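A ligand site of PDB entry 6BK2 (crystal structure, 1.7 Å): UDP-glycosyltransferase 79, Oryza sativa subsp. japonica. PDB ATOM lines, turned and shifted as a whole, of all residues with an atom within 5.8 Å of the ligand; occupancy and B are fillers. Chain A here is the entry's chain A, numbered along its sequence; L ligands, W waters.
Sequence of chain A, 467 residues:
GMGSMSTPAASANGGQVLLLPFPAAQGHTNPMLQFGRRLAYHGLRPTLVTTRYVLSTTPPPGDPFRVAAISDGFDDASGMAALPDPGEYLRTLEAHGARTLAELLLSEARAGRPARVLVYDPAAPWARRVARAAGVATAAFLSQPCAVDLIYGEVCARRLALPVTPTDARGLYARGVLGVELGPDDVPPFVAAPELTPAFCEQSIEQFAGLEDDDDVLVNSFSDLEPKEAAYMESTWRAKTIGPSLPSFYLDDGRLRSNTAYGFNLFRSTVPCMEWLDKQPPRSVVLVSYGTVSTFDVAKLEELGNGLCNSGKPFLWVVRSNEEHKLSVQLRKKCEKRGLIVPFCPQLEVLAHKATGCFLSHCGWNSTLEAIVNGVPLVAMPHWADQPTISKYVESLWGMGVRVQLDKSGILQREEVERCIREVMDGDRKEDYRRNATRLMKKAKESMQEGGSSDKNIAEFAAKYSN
OE1 of Glu 370 sits at hydrogen-bond distance from O3 of the ligand (2.5 Å). An oxygen (O8) of the ligand sits at hydrogen-bond distance from the backbone NH (N) of Ser 367 (3.0 Å). OG of Ser 367 lies within hydrogen-bond range of O8 of the ligand. An oxygen (O11) of the ligand lies within hydrogen-bond range of the backbone NH (N) of Thr 292 (2.8 Å). OG1 of Thr 292 lies within hydrogen-bond range of O11 of the ligand, 2.7 Å away. An oxygen (O2) of the ligand lies within hydrogen-bond range of the backbone NH (N) of Cys 345 (2.9 Å). A nitrogen (N2) of the ligand is in hydrogen-bond range of the backbone carbonyl oxygen (O) of Cys 345. O12 of the ligand lies within hydrogen-bond range of NE2 of His 28, 2.8 Å away. A ring nitrogen (NE2) of His 362 lies within hydrogen-bond range of an oxygen (O10) of the ligand, 2.8 Å away. N of Asn 366 lies within hydrogen-bond range of O7 of the ligand, at 3.2 Å. ND2 of Asn 366 lies within hydrogen-bond range of O7 of the ligand (3.1 Å). An oxygen (O3) of the ligand is in hydrogen-bond range of the side-chain amide nitrogen (NE2) of Gln 347 (3.2 Å).
The side-chain amide nitrogen (NE2) of Gln 347 is in hydrogen-bond range of the side-chain carboxylate (OE1) of Glu 370. NE2 of Gln 347 is in hydrogen-bond range of OG of Ser 367, 3.1 Å away. The backbone NH of His 362 lies within hydrogen-bond range of the backbone carbonyl oxygen of Ser 289 (3.4 Å). The backbone carbonyl oxygen (O) of Gly 364 lies within hydrogen-bond range of the side-chain hydroxyl (OG1) of Thr 368. The side-chain hydroxyl (OG) of Ser 289 sits at hydrogen-bond distance from the backbone NH (N) of Gly 291, 3.2 Å away.
Gly 291 touches the ligand. CG1 of Val 318 touches O2 of the ligand (3.6 Å). Phe 344 touches the ligand (CZ to N2, 3.4 Å). CA of Gly 364 touches O8 of the ligand (3.5 Å). Trp 365 touches the ligand (N to O7, 3.5 Å). Within 4 Å of the ligand: His 28, Gly 291, Thr 292, Val 318, Phe 344, Cys 345, Gln 347, His 362, Gly 364, Trp 365, Asn 366, Ser 367 and Glu 370. The nearest printed residue that does not touch the ligand is Val 293 (4.02 Å).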
ATOM      1  N   GLN A  26      12.167 -30.254 -12.292  1.00  0.00           N
ATOM      2  CA  GLN A  26      12.172 -29.934 -10.867  1.00  0.00           C
ATOM      3  C   GLN A  26      13.472 -29.185 -10.429  1.00  0.00           C
ATOM      4  O   GLN A  26      13.545 -28.731  -9.263  1.00  0.00           O
ATOM      5  CB  GLN A  26      12.024 -31.210 -10.010  1.00  0.00           C
ATOM      6  CG  GLN A  26      13.304 -32.052  -9.893  1.00  0.00           C
ATOM      7  CD  GLN A  26      13.215 -33.127  -8.802  1.00  0.00           C
ATOM      8  OE1 GLN A  26      12.157 -33.747  -8.588  1.00  0.00           O
ATOM      9  NE2 GLN A  26      14.322 -33.348  -8.104  1.00  0.00           N
ATOM     10  N   HIS A  28      16.439 -26.192 -10.374  1.00  0.00           N
ATOM     11  CA  HIS A  28      16.310 -24.767 -10.328  1.00  0.00           C
ATOM     12  C   HIS A  28      17.482 -24.125 -11.079  1.00  0.00           C
ATOM     13  O   HIS A  28      18.626 -24.431 -10.803  1.00  0.00           O
ATOM     14  CB  HIS A  28      16.378 -24.296  -8.919  1.00  0.00           C
ATOM     15  CG  HIS A  28      15.289 -24.876  -8.074  1.00  0.00           C
ATOM     16  ND1 HIS A  28      13.957 -24.630  -8.318  1.00  0.00           N
ATOM     17  CD2 HIS A  28      15.349 -25.781  -7.074  1.00  0.00           C
ATOM     18  CE1 HIS A  28      13.228 -25.327  -7.448  1.00  0.00           C
ATOM     19  NE2 HIS A  28      14.045 -26.041  -6.695  1.00  0.00           N
ATOM     20  N   SER A 289       5.573 -22.174   2.521  1.00  0.00           N
ATOM     21  CA  SER A 289       5.796 -22.975   1.323  1.00  0.00           C
ATOM     22  C   SER A 289       6.563 -24.211   1.697  1.00  0.00           C
ATOM     23  O   SER A 289       7.504 -24.107   2.482  1.00  0.00           O
ATOM     24  CB  SER A 289       6.598 -22.152   0.338  1.00  0.00           C
ATOM     25  OG  SER A 289       6.995 -22.966  -0.841  1.00  0.00           O
ATOM     26  N   TYR A 290       6.247 -25.327   1.046  1.00  0.00           N
ATOM     27  CA  TYR A 290       7.013 -26.557   1.236  1.00  0.00           C
ATOM     28  C   TYR A 290       7.723 -26.966  -0.002  1.00  0.00           C
ATOM     29  O   TYR A 290       8.197 -28.118  -0.055  1.00  0.00           O
ATOM     30  CB  TYR A 290       6.188 -27.674   1.863  1.00  0.00           C
ATOM     31  CG  TYR A 290       4.912 -28.131   1.215  1.00  0.00           C
ATOM     32  CD1 TYR A 290       4.914 -28.956   0.101  1.00  0.00           C
ATOM     33  CD2 TYR A 290       3.771 -27.599   1.562  1.00  0.00           C
ATOM     34  CE1 TYR A 290       3.717 -29.384  -0.470  1.00  0.00           C
ATOM     35  CE2 TYR A 290       2.555 -27.960   0.987  1.00  0.00           C
ATOM     36  CZ  TYR A 290       2.529 -28.882  -0.072  1.00  0.00           C
ATOM     37  OH  TYR A 290       1.330 -29.151  -0.721  1.00  0.00           O
ATOM     38  N   GLY A 291       7.898 -26.007  -0.888  1.00  0.00           N
ATOM     39  CA  GLY A 291       8.763 -26.063  -2.014  1.00  0.00           C
ATOM     40  C   GLY A 291       8.068 -26.663  -3.242  1.00  0.00           C
ATOM     41  O   GLY A 291       6.837 -26.646  -3.311  1.00  0.00           O
ATOM     42  N   THR A 292       8.866 -27.078  -4.207  1.00  0.00           N
ATOM     43  CA  THR A 292       8.319 -27.355  -5.543  1.00  0.00           C
ATOM     44  C   THR A 292       8.225 -28.809  -5.840  1.00  0.00           C
ATOM     45  O   THR A 292       7.626 -29.116  -6.851  1.00  0.00           O
ATOM     46  CB  THR A 292       9.209 -26.681  -6.615  1.00  0.00           C
ATOM     47  OG1 THR A 292      10.506 -27.185  -6.489  1.00  0.00           O
ATOM     48  CG2 THR A 292       9.301 -25.204  -6.422  1.00  0.00           C
ATOM     49  N   VAL A 293       8.741 -29.660  -4.979  1.00  0.00           N
ATOM     50  CA  VAL A 293       8.930 -31.091  -5.175  1.00  0.00           C
ATOM     51  C   VAL A 293       8.111 -31.940  -4.204  1.00  0.00           C
ATOM     52  O   VAL A 293       7.440 -32.956  -4.565  1.00  0.00           O
ATOM     53  CB  VAL A 293      10.423 -31.487  -4.895  1.00  0.00           C
ATOM     54  CG1 VAL A 293      10.583 -32.978  -5.111  1.00  0.00           C
ATOM     55  CG2 VAL A 293      11.443 -30.716  -5.722  1.00  0.00           C
ATOM     56  N   SER A 294       8.242 -31.627  -2.917  1.00  0.00           N
ATOM     57  CA  SER A 294       7.542 -32.461  -1.904  1.00  0.00           C
ATOM     58  C   SER A 294       6.070 -32.478  -2.088  1.00  0.00           C
ATOM     59  O   SER A 294       5.491 -31.518  -2.526  1.00  0.00           O
ATOM     60  CB  SER A 294       7.801 -31.962  -0.432  1.00  0.00           C
ATOM     61  OG  SER A 294       9.180 -32.107   0.007  1.00  0.00           O
ATOM     62  N   VAL A 318       1.529 -20.953  -0.261  1.00  0.00           N
ATOM     63  CA  VAL A 318       1.738 -21.495  -1.567  1.00  0.00           C
ATOM     64  C   VAL A 318       1.268 -22.927  -1.572  1.00  0.00           C
ATOM     65  O   VAL A 318       1.870 -23.779  -0.885  1.00  0.00           O
ATOM     66  CB  VAL A 318       3.211 -21.342  -2.049  1.00  0.00           C
ATOM     67  CG1 VAL A 318       3.373 -21.974  -3.400  1.00  0.00           C
ATOM     68  CG2 VAL A 318       3.572 -19.882  -1.961  1.00  0.00           C
ATOM     69  N   PRO A 343      -0.864 -20.590  -6.204  1.00  0.00           N
ATOM     70  CA  PRO A 343      -0.093 -21.715  -6.697  1.00  0.00           C
ATOM     71  C   PRO A 343       1.381 -21.521  -6.787  1.00  0.00           C
ATOM     72  O   PRO A 343       2.129 -22.531  -6.793  1.00  0.00           O
ATOM     73  CB  PRO A 343      -0.688 -22.021  -8.115  1.00  0.00           C
ATOM     74  CG  PRO A 343      -1.367 -20.810  -8.447  1.00  0.00           C
ATOM     75  CD  PRO A 343      -1.777 -20.038  -7.221  1.00  0.00           C
ATOM     76  N   PHE A 344       1.762 -20.264  -6.842  1.00  0.00           N
ATOM     77  CA  PHE A 344       3.189 -19.913  -7.025  1.00  0.00           C
ATOM     78  C   PHE A 344       3.240 -18.455  -6.662  1.00  0.00           C
ATOM     79  O   PHE A 344       2.277 -17.695  -6.832  1.00  0.00           O
ATOM     80  CB  PHE A 344       3.588 -20.100  -8.449  1.00  0.00           C
ATOM     81  CG  PHE A 344       5.097 -20.102  -8.644  1.00  0.00           C
ATOM     82  CD1 PHE A 344       5.826 -21.251  -8.356  1.00  0.00           C
ATOM     83  CD2 PHE A 344       5.711 -19.017  -9.207  1.00  0.00           C
ATOM     84  CE1 PHE A 344       7.231 -21.285  -8.594  1.00  0.00           C
ATOM     85  CE2 PHE A 344       7.096 -19.004  -9.427  1.00  0.00           C
ATOM     86  CZ  PHE A 344       7.846 -20.146  -9.133  1.00  0.00           C
ATOM     87  N   CYS A 345       4.330 -18.050  -6.013  1.00  0.00           N
ATOM     88  CA  CYS A 345       4.506 -16.637  -5.733  1.00  0.00           C
ATOM     89  C   CYS A 345       5.914 -16.176  -6.170  1.00  0.00           C
ATOM     90  O   CYS A 345       6.793 -17.038  -6.352  1.00  0.00           O
ATOM     91  CB  CYS A 345       4.348 -16.396  -4.215  1.00  0.00           C
ATOM     92  SG  CYS A 345       5.661 -16.855  -3.162  1.00  0.00           S
ATOM     93  N   PRO A 346       6.186 -14.883  -6.315  1.00  0.00           N
ATOM     94  CA  PRO A 346       7.566 -14.376  -6.601  1.00  0.00           C
ATOM     95  C   PRO A 346       8.250 -14.301  -5.261  1.00  0.00           C
ATOM     96  O   PRO A 346       8.197 -13.322  -4.523  1.00  0.00           O
ATOM     97  CB  PRO A 346       7.305 -12.999  -7.233  1.00  0.00           C
ATOM     98  CG  PRO A 346       6.059 -12.604  -6.662  1.00  0.00           C
ATOM     99  CD  PRO A 346       5.185 -13.797  -6.447  1.00  0.00           C
ATOM    100  N   GLN A 347       8.823 -15.434  -4.883  1.00  0.00           N
ATOM    101  CA  GLN A 347       9.242 -15.637  -3.504  1.00  0.00           C
ATOM    102  C   GLN A 347      10.248 -14.636  -3.045  1.00  0.00           C
ATOM    103  O   GLN A 347      10.150 -14.148  -1.910  1.00  0.00           O
ATOM    104  CB  GLN A 347       9.736 -17.091  -3.353  1.00  0.00           C
ATOM    105  CG  GLN A 347      10.216 -17.360  -1.965  1.00  0.00           C
ATOM    106  CD  GLN A 347      10.413 -18.876  -1.685  1.00  0.00           C
ATOM    107  OE1 GLN A 347       9.498 -19.643  -1.858  1.00  0.00           O
ATOM    108  NE2 GLN A 347      11.594 -19.234  -1.266  1.00  0.00           N
ATOM    109  N   LEU A 348      11.252 -14.286  -3.882  1.00  0.00           N
ATOM    110  CA  LEU A 348      12.163 -13.213  -3.499  1.00  0.00           C
ATOM    111  C   LEU A 348      11.508 -11.875  -3.229  1.00  0.00           C
ATOM    112  O   LEU A 348      11.771 -11.245  -2.220  1.00  0.00           O
ATOM    113  CB  LEU A 348      13.340 -13.044  -4.471  1.00  0.00           C
ATOM    114  CG  LEU A 348      14.554 -13.947  -4.217  1.00  0.00           C
ATOM    115  CD1 LEU A 348      15.363 -13.727  -5.489  1.00  0.00           C
ATOM    116  CD2 LEU A 348      15.290 -13.501  -2.986  1.00  0.00           C
ATOM    117  N   HIS A 362      10.043 -25.418   4.259  1.00  0.00           N
ATOM    118  CA  HIS A 362      10.671 -26.734   4.366  1.00  0.00           C
ATOM    119  C   HIS A 362      12.219 -26.649   4.481  1.00  0.00           C
ATOM    120  O   HIS A 362      12.860 -27.648   4.733  1.00  0.00           O
ATOM    121  CB  HIS A 362      10.229 -27.601   3.225  1.00  0.00           C
ATOM    122  CG  HIS A 362      10.905 -27.285   1.929  1.00  0.00           C
ATOM    123  ND1 HIS A 362      10.882 -26.014   1.359  1.00  0.00           N
ATOM    124  CD2 HIS A 362      11.495 -28.095   1.039  1.00  0.00           C
ATOM    125  CE1 HIS A 362      11.533 -26.068   0.211  1.00  0.00           C
ATOM    126  NE2 HIS A 362      11.862 -27.349  -0.042  1.00  0.00           N
ATOM    127  N   CYS A 363      12.770 -25.480   4.302  1.00  0.00           N
ATOM    128  CA  CYS A 363      14.207 -25.253   4.487  1.00  0.00           C
ATOM    129  C   CYS A 363      14.992 -25.973   3.397  1.00  0.00           C
ATOM    130  O   CYS A 363      16.083 -26.410   3.655  1.00  0.00           O
ATOM    131  CB  CYS A 363      14.709 -25.473   5.897  1.00  0.00           C
ATOM    132  SG  CYS A 363      14.312 -24.017   6.900  1.00  0.00           S
ATOM    133  N   GLY A 364      14.435 -26.056   2.182  1.00  0.00           N
ATOM    134  CA  GLY A 364      15.222 -26.198   1.015  1.00  0.00           C
ATOM    135  C   GLY A 364      16.330 -25.114   0.963  1.00  0.00           C
ATOM    136  O   GLY A 364      16.183 -24.050   1.521  1.00  0.00           O
ATOM    137  N   TRP A 365      17.495 -25.450   0.377  1.00  0.00           N
ATOM    138  CA  TRP A 365      18.599 -24.478   0.501  1.00  0.00           C
ATOM    139  C   TRP A 365      18.311 -23.208  -0.216  1.00  0.00           C
ATOM    140  O   TRP A 365      18.717 -22.130   0.286  1.00  0.00           O
ATOM    141  CB  TRP A 365      19.844 -25.097   0.007  1.00  0.00           C
ATOM    142  CG  TRP A 365      21.082 -24.342   0.209  1.00  0.00           C
ATOM    143  CD1 TRP A 365      22.084 -24.023  -0.755  1.00  0.00           C
ATOM    144  CD2 TRP A 365      21.580 -23.796   1.430  1.00  0.00           C
ATOM    145  NE1 TRP A 365      23.085 -23.397  -0.161  1.00  0.00           N
ATOM    146  CE2 TRP A 365      22.852 -23.224   1.171  1.00  0.00           C
ATOM    147  CE3 TRP A 365      21.090 -23.749   2.720  1.00  0.00           C
ATOM    148  CZ2 TRP A 365      23.563 -22.619   2.122  1.00  0.00           C
ATOM    149  CZ3 TRP A 365      21.857 -23.137   3.703  1.00  0.00           C
ATOM    150  CH2 TRP A 365      23.102 -22.588   3.370  1.00  0.00           C
ATOM    151  N   ASN A 366      17.730 -23.265  -1.410  1.00  0.00           N
ATOM    152  CA  ASN A 366      17.431 -21.963  -2.078  1.00  0.00           C
ATOM    153  C   ASN A 366      16.490 -21.142  -1.263  1.00  0.00           C
ATOM    154  O   ASN A 366      16.739 -19.925  -1.102  1.00  0.00           O
ATOM    155  CB  ASN A 366      16.923 -22.163  -3.500  1.00  0.00           C
ATOM    156  CG  ASN A 366      17.926 -22.875  -4.336  1.00  0.00           C
ATOM    157  OD1 ASN A 366      19.038 -22.410  -4.469  1.00  0.00           O
ATOM    158  ND2 ASN A 366      17.595 -24.055  -4.805  1.00  0.00           N
ATOM    159  N   SER A 367      15.452 -21.687  -0.684  1.00  0.00           N
ATOM    160  CA  SER A 367      14.525 -20.912   0.145  1.00  0.00           C
ATOM    161  C   SER A 367      15.208 -20.347   1.369  1.00  0.00           C
ATOM    162  O   SER A 367      14.977 -19.231   1.820  1.00  0.00           O
ATOM    163  CB  SER A 367      13.281 -21.766   0.565  1.00  0.00           C
ATOM    164  OG  SER A 367      12.516 -22.089  -0.584  1.00  0.00           O
ATOM    165  N   THR A 368      16.131 -21.096   1.949  1.00  0.00           N
ATOM    166  CA  THR A 368      16.855 -20.667   3.142  1.00  0.00           C
ATOM    167  C   THR A 368      17.767 -19.480   2.831  1.00  0.00           C
ATOM    168  O   THR A 368      17.778 -18.474   3.557  1.00  0.00           O
ATOM    169  CB  THR A 368      17.677 -21.807   3.751  1.00  0.00           C
ATOM    170  OG1 THR A 368      16.735 -22.901   4.026  1.00  0.00           O
ATOM    171  CG2 THR A 368      18.377 -21.358   5.017  1.00  0.00           C
ATOM    172  N   GLU A 370      17.357 -17.387   0.421  1.00  0.00           N
ATOM    173  CA  GLU A 370      16.470 -16.241   0.125  1.00  0.00           C
ATOM    174  C   GLU A 370      15.958 -15.609   1.391  1.00  0.00           C
ATOM    175  O   GLU A 370      15.865 -14.357   1.503  1.00  0.00           O
ATOM    176  CB  GLU A 370      15.378 -16.682  -0.844  1.00  0.00           C
ATOM    177  CG  GLU A 370      15.942 -17.100  -2.213  1.00  0.00           C
ATOM    178  CD  GLU A 370      15.056 -17.970  -3.008  1.00  0.00           C
ATOM    179  OE1 GLU A 370      13.847 -18.080  -2.639  1.00  0.00           O
ATOM    180  OE2 GLU A 370      15.550 -18.530  -4.077  1.00  0.00           O
ATOM    181  N   GLN A 387      17.409 -30.761   4.129  1.00  0.00           N
ATOM    182  CA  GLN A 387      16.571 -29.949   4.982  1.00  0.00           C
ATOM    183  C   GLN A 387      16.644 -30.180   6.441  1.00  0.00           C
ATOM    184  O   GLN A 387      16.649 -29.203   7.211  1.00  0.00           O
ATOM    185  CB  GLN A 387      15.090 -30.087   4.488  1.00  0.00           C
ATOM    186  CG  GLN A 387      14.851 -29.692   3.053  1.00  0.00           C
ATOM    187  CD  GLN A 387      13.831 -30.532   2.323  1.00  0.00           C
ATOM    188  OE1 GLN A 387      12.932 -31.097   2.947  1.00  0.00           O
ATOM    189  NE2 GLN A 387      13.941 -30.606   0.976  1.00  0.00           N
HETATM  190  N1  LIG L   1       9.927 -20.672  -5.516  1.00  0.00           N
HETATM  191  C1  LIG L   1       9.258 -19.540  -5.972  1.00  0.00           C
HETATM  192  N2  LIG L   1       7.930 -19.467  -5.780  1.00  0.00           N
HETATM  193  C2  LIG L   1       7.215 -20.384  -5.110  1.00  0.00           C
HETATM  194  C3  LIG L   1       7.846 -21.556  -4.634  1.00  0.00           C
HETATM  195  C4  LIG L   1       9.199 -21.613  -4.841  1.00  0.00           C
HETATM  196  O1  LIG L   1       9.853 -18.671  -6.559  1.00  0.00           O
HETATM  197  O2  LIG L   1       5.998 -20.182  -4.988  1.00  0.00           O
HETATM  198  C5  LIG L   1      11.370 -20.726  -5.746  1.00  0.00           C
HETATM  199  C6  LIG L   1      12.084 -20.366  -4.472  1.00  0.00           C
HETATM  200  O3  LIG L   1      12.275 -18.909  -4.341  1.00  0.00           O
HETATM  201  C7  LIG L   1      13.382 -21.185  -4.645  1.00  0.00           C
HETATM  202  C8  LIG L   1      12.940 -22.474  -5.331  1.00  0.00           C
HETATM  203  O4  LIG L   1      11.648 -22.137  -5.885  1.00  0.00           O
HETATM  204  O5  LIG L   1      14.322 -20.468  -5.475  1.00  0.00           O
HETATM  205  C9  LIG L   1      12.664 -23.631  -4.358  1.00  0.00           C
HETATM  206  O6  LIG L   1      13.954 -24.214  -4.018  1.00  0.00           O
HETATM  207  P1  LIG L   1      14.248 -24.912  -2.668  1.00  0.00           P
HETATM  208  O7  LIG L   1      15.691 -25.333  -2.662  1.00  0.00           O
HETATM  209  O8  LIG L   1      13.914 -24.114  -1.516  1.00  0.00           O
HETATM  210  O9  LIG L   1      13.406 -26.281  -2.538  1.00  0.00           O
HETATM  211  P2  LIG L   1      12.730 -27.327  -3.544  1.00  0.00           P
HETATM  212  O10 LIG L   1      12.467 -28.388  -2.594  1.00  0.00           O
HETATM  213  O11 LIG L   1      11.584 -26.650  -4.127  1.00  0.00           O
HETATM  214  O12 LIG L   1      13.857 -27.744  -4.492  1.00  0.00           O
HETATM  215  O   HOH W   1       9.844 -29.328  -2.099  1.00  0.00           O
HETATM  216  O   HOH W   2      16.204 -20.961  -7.167  1.00  0.00           O
HETATM  217  O   HOH W   3       9.581 -16.625  -8.464  1.00  0.00           O
